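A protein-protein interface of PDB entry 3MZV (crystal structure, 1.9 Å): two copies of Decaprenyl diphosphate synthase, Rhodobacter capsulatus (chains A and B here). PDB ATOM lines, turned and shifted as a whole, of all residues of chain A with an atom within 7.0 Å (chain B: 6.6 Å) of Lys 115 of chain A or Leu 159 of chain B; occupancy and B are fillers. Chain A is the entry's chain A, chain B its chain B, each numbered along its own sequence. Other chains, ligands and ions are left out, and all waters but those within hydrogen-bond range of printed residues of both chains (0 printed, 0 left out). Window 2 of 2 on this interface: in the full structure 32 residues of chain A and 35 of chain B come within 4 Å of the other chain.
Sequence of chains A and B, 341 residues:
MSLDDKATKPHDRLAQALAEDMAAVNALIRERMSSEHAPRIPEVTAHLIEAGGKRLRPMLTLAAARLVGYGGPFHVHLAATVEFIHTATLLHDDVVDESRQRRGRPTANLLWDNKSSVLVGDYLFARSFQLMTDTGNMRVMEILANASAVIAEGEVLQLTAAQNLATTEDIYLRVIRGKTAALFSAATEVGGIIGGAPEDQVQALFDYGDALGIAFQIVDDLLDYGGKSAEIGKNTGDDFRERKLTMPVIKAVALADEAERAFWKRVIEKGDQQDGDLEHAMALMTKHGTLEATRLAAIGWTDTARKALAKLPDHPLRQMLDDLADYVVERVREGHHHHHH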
ATOM      1  N   ARG A  40      17.557  20.681  26.018  1.00  0.00           N
ATOM      2  CA  ARG A  40      17.579  22.013  25.379  1.00  0.00           C
ATOM      3  C   ARG A  40      18.422  22.039  24.092  1.00  0.00           C
ATOM      4  O   ARG A  40      18.049  22.692  23.109  1.00  0.00           O
ATOM      5  CB  ARG A  40      18.081  23.066  26.374  1.00  0.00           C
ATOM      6  CG  ARG A  40      18.122  24.483  25.828  1.00  0.00           C
ATOM      7  CD  ARG A  40      18.469  25.491  26.903  1.00  0.00           C
ATOM      8  NE  ARG A  40      17.425  25.582  27.924  1.00  0.00           N
ATOM      9  CZ  ARG A  40      17.417  26.467  28.920  1.00  0.00           C
ATOM     10  NH1 ARG A  40      18.390  27.362  29.041  1.00  0.00           N
ATOM     11  NH2 ARG A  40      16.426  26.464  29.805  1.00  0.00           N
ATOM     12  N   VAL A  95      23.535  36.637  18.864  1.00  0.00           N
ATOM     13  CA  VAL A  95      23.722  37.219  20.165  1.00  0.00           C
ATOM     14  C   VAL A  95      24.274  38.610  19.956  1.00  0.00           C
ATOM     15  O   VAL A  95      23.773  39.497  20.602  1.00  0.00           O
ATOM     16  CB  VAL A  95      24.637  36.433  21.139  1.00  0.00           C
ATOM     17  CG1 VAL A  95      24.503  34.964  20.962  1.00  0.00           C
ATOM     18  CG2 VAL A  95      26.073  36.887  20.986  1.00  0.00           C
ATOM     19  N   ASN A 109      17.987  33.035  21.066  1.00  0.00           N
ATOM     20  CA  ASN A 109      18.414  33.928  22.137  1.00  0.00           C
ATOM     21  C   ASN A 109      17.240  34.657  22.769  1.00  0.00           C
ATOM     22  O   ASN A 109      17.303  35.008  23.940  1.00  0.00           O
ATOM     23  CB  ASN A 109      19.495  34.937  21.692  1.00  0.00           C
ATOM     24  CG  ASN A 109      19.133  35.673  20.407  1.00  0.00           C
ATOM     25  OD1 ASN A 109      19.336  35.154  19.304  1.00  0.00           O
ATOM     26  ND2 ASN A 109      18.601  36.888  20.549  1.00  0.00           N
ATOM     27  N   TRP A 112      14.932  31.381  24.503  1.00  0.00           N
ATOM     28  CA  TRP A 112      15.627  31.115  25.765  1.00  0.00           C
ATOM     29  C   TRP A 112      16.394  32.384  26.165  1.00  0.00           C
ATOM     30  O   TRP A 112      15.787  33.299  26.724  1.00  0.00           O
ATOM     31  CB  TRP A 112      16.524  29.890  25.626  1.00  0.00           C
ATOM     32  CG  TRP A 112      15.759  28.650  25.254  1.00  0.00           C
ATOM     33  CD1 TRP A 112      15.247  27.719  26.115  1.00  0.00           C
ATOM     34  CD2 TRP A 112      15.400  28.215  23.931  1.00  0.00           C
ATOM     35  NE1 TRP A 112      14.601  26.725  25.409  1.00  0.00           N
ATOM     36  CE2 TRP A 112      14.678  27.006  24.069  1.00  0.00           C
ATOM     37  CE3 TRP A 112      15.614  28.730  22.644  1.00  0.00           C
ATOM     38  CZ2 TRP A 112      14.167  26.301  22.968  1.00  0.00           C
ATOM     39  CZ3 TRP A 112      15.105  28.029  21.547  1.00  0.00           C
ATOM     40  CH2 TRP A 112      14.393  26.825  21.717  1.00  0.00           C
ATOM     41  N   ASP A 113      17.690  32.469  25.854  1.00  0.00           N
ATOM     42  CA  ASP A 113      18.489  33.657  26.174  1.00  0.00           C
ATOM     43  C   ASP A 113      19.815  33.685  25.358  1.00  0.00           C
ATOM     44  O   ASP A 113      20.142  32.698  24.671  1.00  0.00           O
ATOM     45  CB  ASP A 113      18.730  33.707  27.681  1.00  0.00           C
ATOM     46  N   ASN A 114      20.541  34.818  25.368  1.00  0.00           N
ATOM     47  CA  ASN A 114      21.914  34.893  24.795  1.00  0.00           C
ATOM     48  C   ASN A 114      22.709  33.688  25.277  1.00  0.00           C
ATOM     49  O   ASN A 114      23.494  33.096  24.542  1.00  0.00           O
ATOM     50  CB  ASN A 114      22.670  36.144  25.279  1.00  0.00           C
ATOM     51  CG  ASN A 114      22.563  37.340  24.337  1.00  0.00           C
ATOM     52  OD1 ASN A 114      23.049  38.422  24.678  1.00  0.00           O
ATOM     53  ND2 ASN A 114      21.964  37.163  23.165  1.00  0.00           N
ATOM     54  N   LYS A 115      22.496  33.371  26.548  1.00  0.00           N
ATOM     55  CA  LYS A 115      23.027  32.192  27.211  1.00  0.00           C
ATOM     56  C   LYS A 115      22.893  30.922  26.364  1.00  0.00           C
ATOM     57  O   LYS A 115      23.880  30.223  26.172  1.00  0.00           O
ATOM     58  CB  LYS A 115      22.305  31.933  28.540  1.00  0.00           C
ATOM     59  CG  LYS A 115      21.697  33.128  29.293  1.00  0.00           C
ATOM     60  CD  LYS A 115      21.115  32.620  30.618  1.00  0.00           C
ATOM     61  CE  LYS A 115      21.153  33.672  31.707  1.00  0.00           C
ATOM     62  NZ  LYS A 115      21.231  33.064  33.083  1.00  0.00           N
ATOM     63  N   SER A 116      21.680  30.682  25.856  1.00  0.00           N
ATOM     64  CA  SER A 116      21.349  29.540  24.970  1.00  0.00           C
ATOM     65  C   SER A 116      21.918  29.615  23.574  1.00  0.00           C
ATOM     66  O   SER A 116      22.458  28.639  23.087  1.00  0.00           O
ATOM     67  CB  SER A 116      19.819  29.335  24.886  1.00  0.00           C
ATOM     68  OG  SER A 116      19.169  30.285  24.046  1.00  0.00           O
ATOM     69  N   SER A 117      21.795  30.728  22.874  1.00  0.00           N
ATOM     70  CA  SER A 117      22.504  30.813  21.641  1.00  0.00           C
ATOM     71  C   SER A 117      23.981  30.416  21.888  1.00  0.00           C
ATOM     72  O   SER A 117      24.533  29.586  21.170  1.00  0.00           O
ATOM     73  CB  SER A 117      22.415  32.198  21.058  1.00  0.00           C
ATOM     74  OG  SER A 117      21.059  32.595  20.918  1.00  0.00           O
ATOM     75  N   VAL A 118      24.617  31.000  22.909  1.00  0.00           N
ATOM     76  CA  VAL A 118      26.061  30.850  23.032  1.00  0.00           C
ATOM     77  C   VAL A 118      26.416  29.395  23.309  1.00  0.00           C
ATOM     78  O   VAL A 118      27.238  28.822  22.624  1.00  0.00           O
ATOM     79  CB  VAL A 118      26.688  31.821  24.094  1.00  0.00           C
ATOM     80  CG1 VAL A 118      28.156  31.488  24.226  1.00  0.00           C
ATOM     81  CG2 VAL A 118      26.502  33.293  23.665  1.00  0.00           C
ATOM     82  N   LEU A 119      25.770  28.778  24.291  1.00  0.00           N
ATOM     83  CA  LEU A 119      26.148  27.450  24.737  1.00  0.00           C
ATOM     84  C   LEU A 119      25.759  26.355  23.769  1.00  0.00           C
ATOM     85  O   LEU A 119      26.544  25.481  23.536  1.00  0.00           O
ATOM     86  CB  LEU A 119      25.584  27.168  26.141  1.00  0.00           C
ATOM     87  CG  LEU A 119      26.227  28.041  27.226  1.00  0.00           C
ATOM     88  CD1 LEU A 119      25.489  27.780  28.528  1.00  0.00           C
ATOM     89  CD2 LEU A 119      27.750  27.849  27.359  1.00  0.00           C
ATOM     90  N   VAL A 120      24.609  26.456  23.128  1.00  0.00           N
ATOM     91  CA  VAL A 120      24.249  25.477  22.104  1.00  0.00           C
ATOM     92  C   VAL A 120      25.227  25.581  20.906  1.00  0.00           C
ATOM     93  O   VAL A 120      25.715  24.567  20.381  1.00  0.00           O
ATOM     94  CB  VAL A 120      22.793  25.626  21.661  1.00  0.00           C
ATOM     95  CG1 VAL A 120      22.505  24.662  20.441  1.00  0.00           C
ATOM     96  CG2 VAL A 120      21.806  25.397  22.841  1.00  0.00           C
ATOM     97  N   GLY A 121      25.506  26.801  20.467  1.00  0.00           N
ATOM     98  CA  GLY A 121      26.497  27.004  19.418  1.00  0.00           C
ATOM     99  C   GLY A 121      27.819  26.332  19.774  1.00  0.00           C
ATOM    100  O   GLY A 121      28.431  25.669  18.905  1.00  0.00           O
ATOM    101  N   VAL B  95      29.738  36.177  29.052  1.00  0.00           N
ATOM    102  CA  VAL B  95      28.598  36.640  28.276  1.00  0.00           C
ATOM    103  C   VAL B  95      27.328  36.046  28.882  1.00  0.00           C
ATOM    104  O   VAL B  95      26.385  36.780  29.199  1.00  0.00           O
ATOM    105  CB  VAL B  95      28.741  36.279  26.784  1.00  0.00           C
ATOM    106  CG1 VAL B  95      27.462  36.622  26.014  1.00  0.00           C
ATOM    107  CG2 VAL B  95      29.926  37.052  26.188  1.00  0.00           C
ATOM    108  N   VAL B  96      27.346  34.731  29.103  1.00  0.00           N
ATOM    109  CA  VAL B  96      26.191  33.960  29.608  1.00  0.00           C
ATOM    110  C   VAL B  96      25.559  34.561  30.905  1.00  0.00           C
ATOM    111  O   VAL B  96      24.360  34.897  30.910  1.00  0.00           O
ATOM    112  CB  VAL B  96      26.568  32.442  29.744  1.00  0.00           C
ATOM    113  CG1 VAL B  96      25.590  31.661  30.596  1.00  0.00           C
ATOM    114  CG2 VAL B  96      26.663  31.813  28.344  1.00  0.00           C
ATOM    115  N   ASP B  97      26.331  34.710  31.985  1.00  0.00           N
ATOM    116  CA  ASP B  97      25.802  35.422  33.191  1.00  0.00           C
ATOM    117  C   ASP B  97      26.076  36.957  33.206  1.00  0.00           C
ATOM    118  O   ASP B  97      25.850  37.637  34.221  1.00  0.00           O
ATOM    119  CB  ASP B  97      26.209  34.719  34.516  1.00  0.00           C
ATOM    120  CG  ASP B  97      27.706  34.556  34.687  1.00  0.00           C
ATOM    121  OD1 ASP B  97      28.454  35.483  34.337  1.00  0.00           O
ATOM    122  OD2 ASP B  97      28.144  33.496  35.189  1.00  0.00           O
ATOM    123  N   GLU B  98      26.498  37.488  32.052  1.00  0.00           N
ATOM    124  CA  GLU B  98      26.740  38.921  31.830  1.00  0.00           C
ATOM    125  C   GLU B  98      27.522  39.537  33.022  1.00  0.00           C
ATOM    126  O   GLU B  98      27.025  40.422  33.744  1.00  0.00           O
ATOM    127  CB  GLU B  98      25.418  39.646  31.457  1.00  0.00           C
ATOM    128  CG  GLU B  98      25.167  39.825  29.915  1.00  0.00           C
ATOM    129  CD  GLU B  98      24.254  38.749  29.225  1.00  0.00           C
ATOM    130  OE1 GLU B  98      23.569  37.973  29.932  1.00  0.00           O
ATOM    131  OE2 GLU B  98      24.209  38.695  27.955  1.00  0.00           O
ATOM    132  N   GLY B 154      27.533  20.745  30.336  1.00  0.00           N
ATOM    133  CA  GLY B 154      27.545  20.940  31.806  1.00  0.00           C
ATOM    134  C   GLY B 154      27.052  22.332  32.187  1.00  0.00           C
ATOM    135  O   GLY B 154      26.258  22.497  33.136  1.00  0.00           O
ATOM    136  N   GLU B 155      27.465  23.331  31.416  1.00  0.00           N
ATOM    137  CA  GLU B 155      26.960  24.681  31.581  1.00  0.00           C
ATOM    138  C   GLU B 155      25.465  24.830  31.299  1.00  0.00           C
ATOM    139  O   GLU B 155      24.761  25.521  32.013  1.00  0.00           O
ATOM    140  CB  GLU B 155      27.797  25.656  30.739  1.00  0.00           C
ATOM    141  CG  GLU B 155      29.244  25.726  31.312  1.00  0.00           C
ATOM    142  CD  GLU B 155      30.139  26.777  30.664  1.00  0.00           C
ATOM    143  OE1 GLU B 155      29.742  27.368  29.641  1.00  0.00           O
ATOM    144  OE2 GLU B 155      31.252  27.016  31.192  1.00  0.00           O
ATOM    145  N   VAL B 156      24.934  24.173  30.261  1.00  0.00           N
ATOM    146  CA  VAL B 156      23.488  24.166  30.065  1.00  0.00           C
ATOM    147  C   VAL B 156      22.756  23.415  31.198  1.00  0.00           C
ATOM    148  O   VAL B 156      21.674  23.850  31.675  1.00  0.00           O
ATOM    149  CB  VAL B 156      23.117  23.538  28.726  1.00  0.00           C
ATOM    150  CG1 VAL B 156      21.604  23.433  28.585  1.00  0.00           C
ATOM    151  CG2 VAL B 156      23.672  24.413  27.616  1.00  0.00           C
ATOM    152  N   LEU B 157      23.309  22.287  31.621  1.00  0.00           N
ATOM    153  CA  LEU B 157      22.757  21.591  32.787  1.00  0.00           C
ATOM    154  C   LEU B 157      22.736  22.479  34.050  1.00  0.00           C
ATOM    155  O   LEU B 157      21.756  22.459  34.814  1.00  0.00           O
ATOM    156  CB  LEU B 157      23.521  20.302  33.070  1.00  0.00           C
ATOM    157  CG  LEU B 157      22.892  19.419  34.169  1.00  0.00           C
ATOM    158  CD1 LEU B 157      21.356  19.166  33.958  1.00  0.00           C
ATOM    159  CD2 LEU B 157      23.617  18.115  34.260  1.00  0.00           C
ATOM    160  N   GLN B 158      23.791  23.256  34.256  1.00  0.00           N
ATOM    161  CA  GLN B 158      23.888  24.123  35.409  1.00  0.00           C
ATOM    162  C   GLN B 158      22.735  25.134  35.406  1.00  0.00           C
ATOM    163  O   GLN B 158      22.202  25.471  36.480  1.00  0.00           O
ATOM    164  CB  GLN B 158      25.239  24.865  35.412  1.00  0.00           C
ATOM    165  CG  GLN B 158      25.451  25.758  36.615  1.00  0.00           C
ATOM    166  CD  GLN B 158      26.836  26.334  36.677  1.00  0.00           C
ATOM    167  OE1 GLN B 158      27.529  26.222  37.693  1.00  0.00           O
ATOM    168  NE2 GLN B 158      27.278  26.942  35.565  1.00  0.00           N
ATOM    169  N   LEU B 159      22.385  25.625  34.208  1.00  0.00           N
ATOM    170  CA  LEU B 159      21.255  26.542  34.039  1.00  0.00           C
ATOM    171  C   LEU B 159      19.904  25.932  34.400  1.00  0.00           C
ATOM    172  O   LEU B 159      19.097  26.588  35.027  1.00  0.00           O
ATOM    173  CB  LEU B 159      21.159  27.046  32.607  1.00  0.00           C
ATOM    174  CG  LEU B 159      22.171  28.101  32.216  1.00  0.00           C
ATOM    175  CD1 LEU B 159      22.019  28.376  30.741  1.00  0.00           C
ATOM    176  CD2 LEU B 159      22.003  29.381  33.071  1.00  0.00           C
ATOM    177  N   THR B 160      19.641  24.699  33.983  1.00  0.00           N
ATOM    178  CA  THR B 160      18.368  24.049  34.297  1.00  0.00           C
ATOM    179  C   THR B 160      18.319  23.592  35.747  1.00  0.00           C
ATOM    180  O   THR B 160      17.264  23.575  36.378  1.00  0.00           O
ATOM    181  CB  THR B 160      18.155  22.821  33.405  1.00  0.00           C
ATOM    182  OG1 THR B 160      19.268  21.930  33.558  1.00  0.00           O
ATOM    183  CG2 THR B 160      18.020  23.255  31.966  1.00  0.00           C
ATOM    184  N   ALA B 161      19.475  23.242  36.294  1.00  0.00           N
ATOM    185  CA  ALA B 161      19.563  22.865  37.682  1.00  0.00           C
ATOM    186  C   ALA B 161      19.331  24.052  38.643  1.00  0.00           C
ATOM    187  O   ALA B 161      19.017  23.840  39.808  1.00  0.00           O
ATOM    188  CB  ALA B 161      20.932  22.246  37.954  1.00  0.00           C
ATOM    189  N   ALA B 162      19.563  25.281  38.191  1.00  0.00           N
ATOM    190  CA  ALA B 162      19.541  26.425  39.102  1.00  0.00           C
ATOM    191  C   ALA B 162      18.077  26.773  39.342  1.00  0.00           C
ATOM    192  O   ALA B 162      17.208  26.505  38.475  1.00  0.00           O
ATOM    193  CB  ALA B 162      20.289  27.620  38.505  1.00  0.00           C
ATOM    194  N   GLN B 163      17.800  27.388  40.491  1.00  0.00           N
ATOM    195  CA  GLN B 163      16.437  27.777  40.847  1.00  0.00           C
ATOM    196  C   GLN B 163      15.561  26.599  41.071  1.00  0.00           C
ATOM    197  O   GLN B 163      14.383  26.776  41.235  1.00  0.00           O
ATOM    198  CB  GLN B 163      15.771  28.660  39.757  1.00  0.00           C
ATOM    199  CG  GLN B 163      16.604  29.877  39.392  1.00  0.00           C
ATOM    200  CD  GLN B 163      15.989  30.759  38.302  1.00  0.00           C
ATOM    201  OE1 GLN B 163      14.842  30.587  37.893  1.00  0.00           O
ATOM    202  NE2 GLN B 163      16.748  31.733  37.873  1.00  0.00           N
ATOM    203  N   VAL B 175      27.028  18.236  36.744  1.00  0.00           N
ATOM    204  CA  VAL B 175      27.299  19.603  36.361  1.00  0.00           C
ATOM    205  C   VAL B 175      28.761  19.905  36.567  1.00  0.00           C
ATOM    206  O   VAL B 175      29.416  20.489  35.693  1.00  0.00           O
ATOM    207  CB  VAL B 175      26.481  20.620  37.177  1.00  0.00           C
ATOM    208  CG1 VAL B 175      27.103  22.016  37.096  1.00  0.00           C
ATOM    209  CG2 VAL B 175      24.984  20.582  36.749  1.00  0.00           C
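The side-chain amide oxygen (OD1) of Asn 114 of chain A lies close to the side-chain carboxylate (OE2) of Glu 98 of chain B (3.5 Å).
Among the printed residues, merely in contact across the chains: Lys 115 of chain A with Val 96 of chain B (3.5 Å), Lys 115 of chain A with Leu 159 of chain B (3.8 Å), Leu 119 of chain A with Val 96 of chain B (3.96 Å), Leu 119 of chain A with Glu 155 of chain B (3.1 Å) and Leu 119 of chain A with Val 156 of chain B (3.7 Å).
Of the printed residues of chain B, Lys 115 of chain A touches Val 96 (3.5 Å) and Leu 159 (3.8 Å).
Of the printed residues of chain B, Asn 114 of chain A touches Glu 98 (3.5 Å).
Of the printed residues of chain A, Glu 155 of chain B touches Leu 119 (3.1 Å).
Printed residues of chain A within 4 Å of Val 96 of chain B: Lys 115 (3.5 Å) and Leu 119 (3.96 Å).
The nearest residue of chain B that does not touch Lys 115 of chain A is Asp 97 of chain B (5.1 Å).
Hydrophobic or aromatic side chains of chain B within 4 Å of the printed part of chain A: Val 96, Val 156 and Leu 159.
Printed residues of chain A that touch a printed residue of chain B: Asn 114, Lys 115 and Leu 119.
Hydrophobic or aromatic side chains of chain A that line the printed part of chain B: Leu 119.
Among the printed residues, 6 pairs touch across the chains.
Among the printed residues, no Asp or Glu carboxylate lies within 4 Å of a Lys or Arg side-chain nitrogen of the other chain.
1 position is printed for both chains.
Of the 6 pairs that touch across the chains among the printed residues, none has its exchanged pair printed and touching as well.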
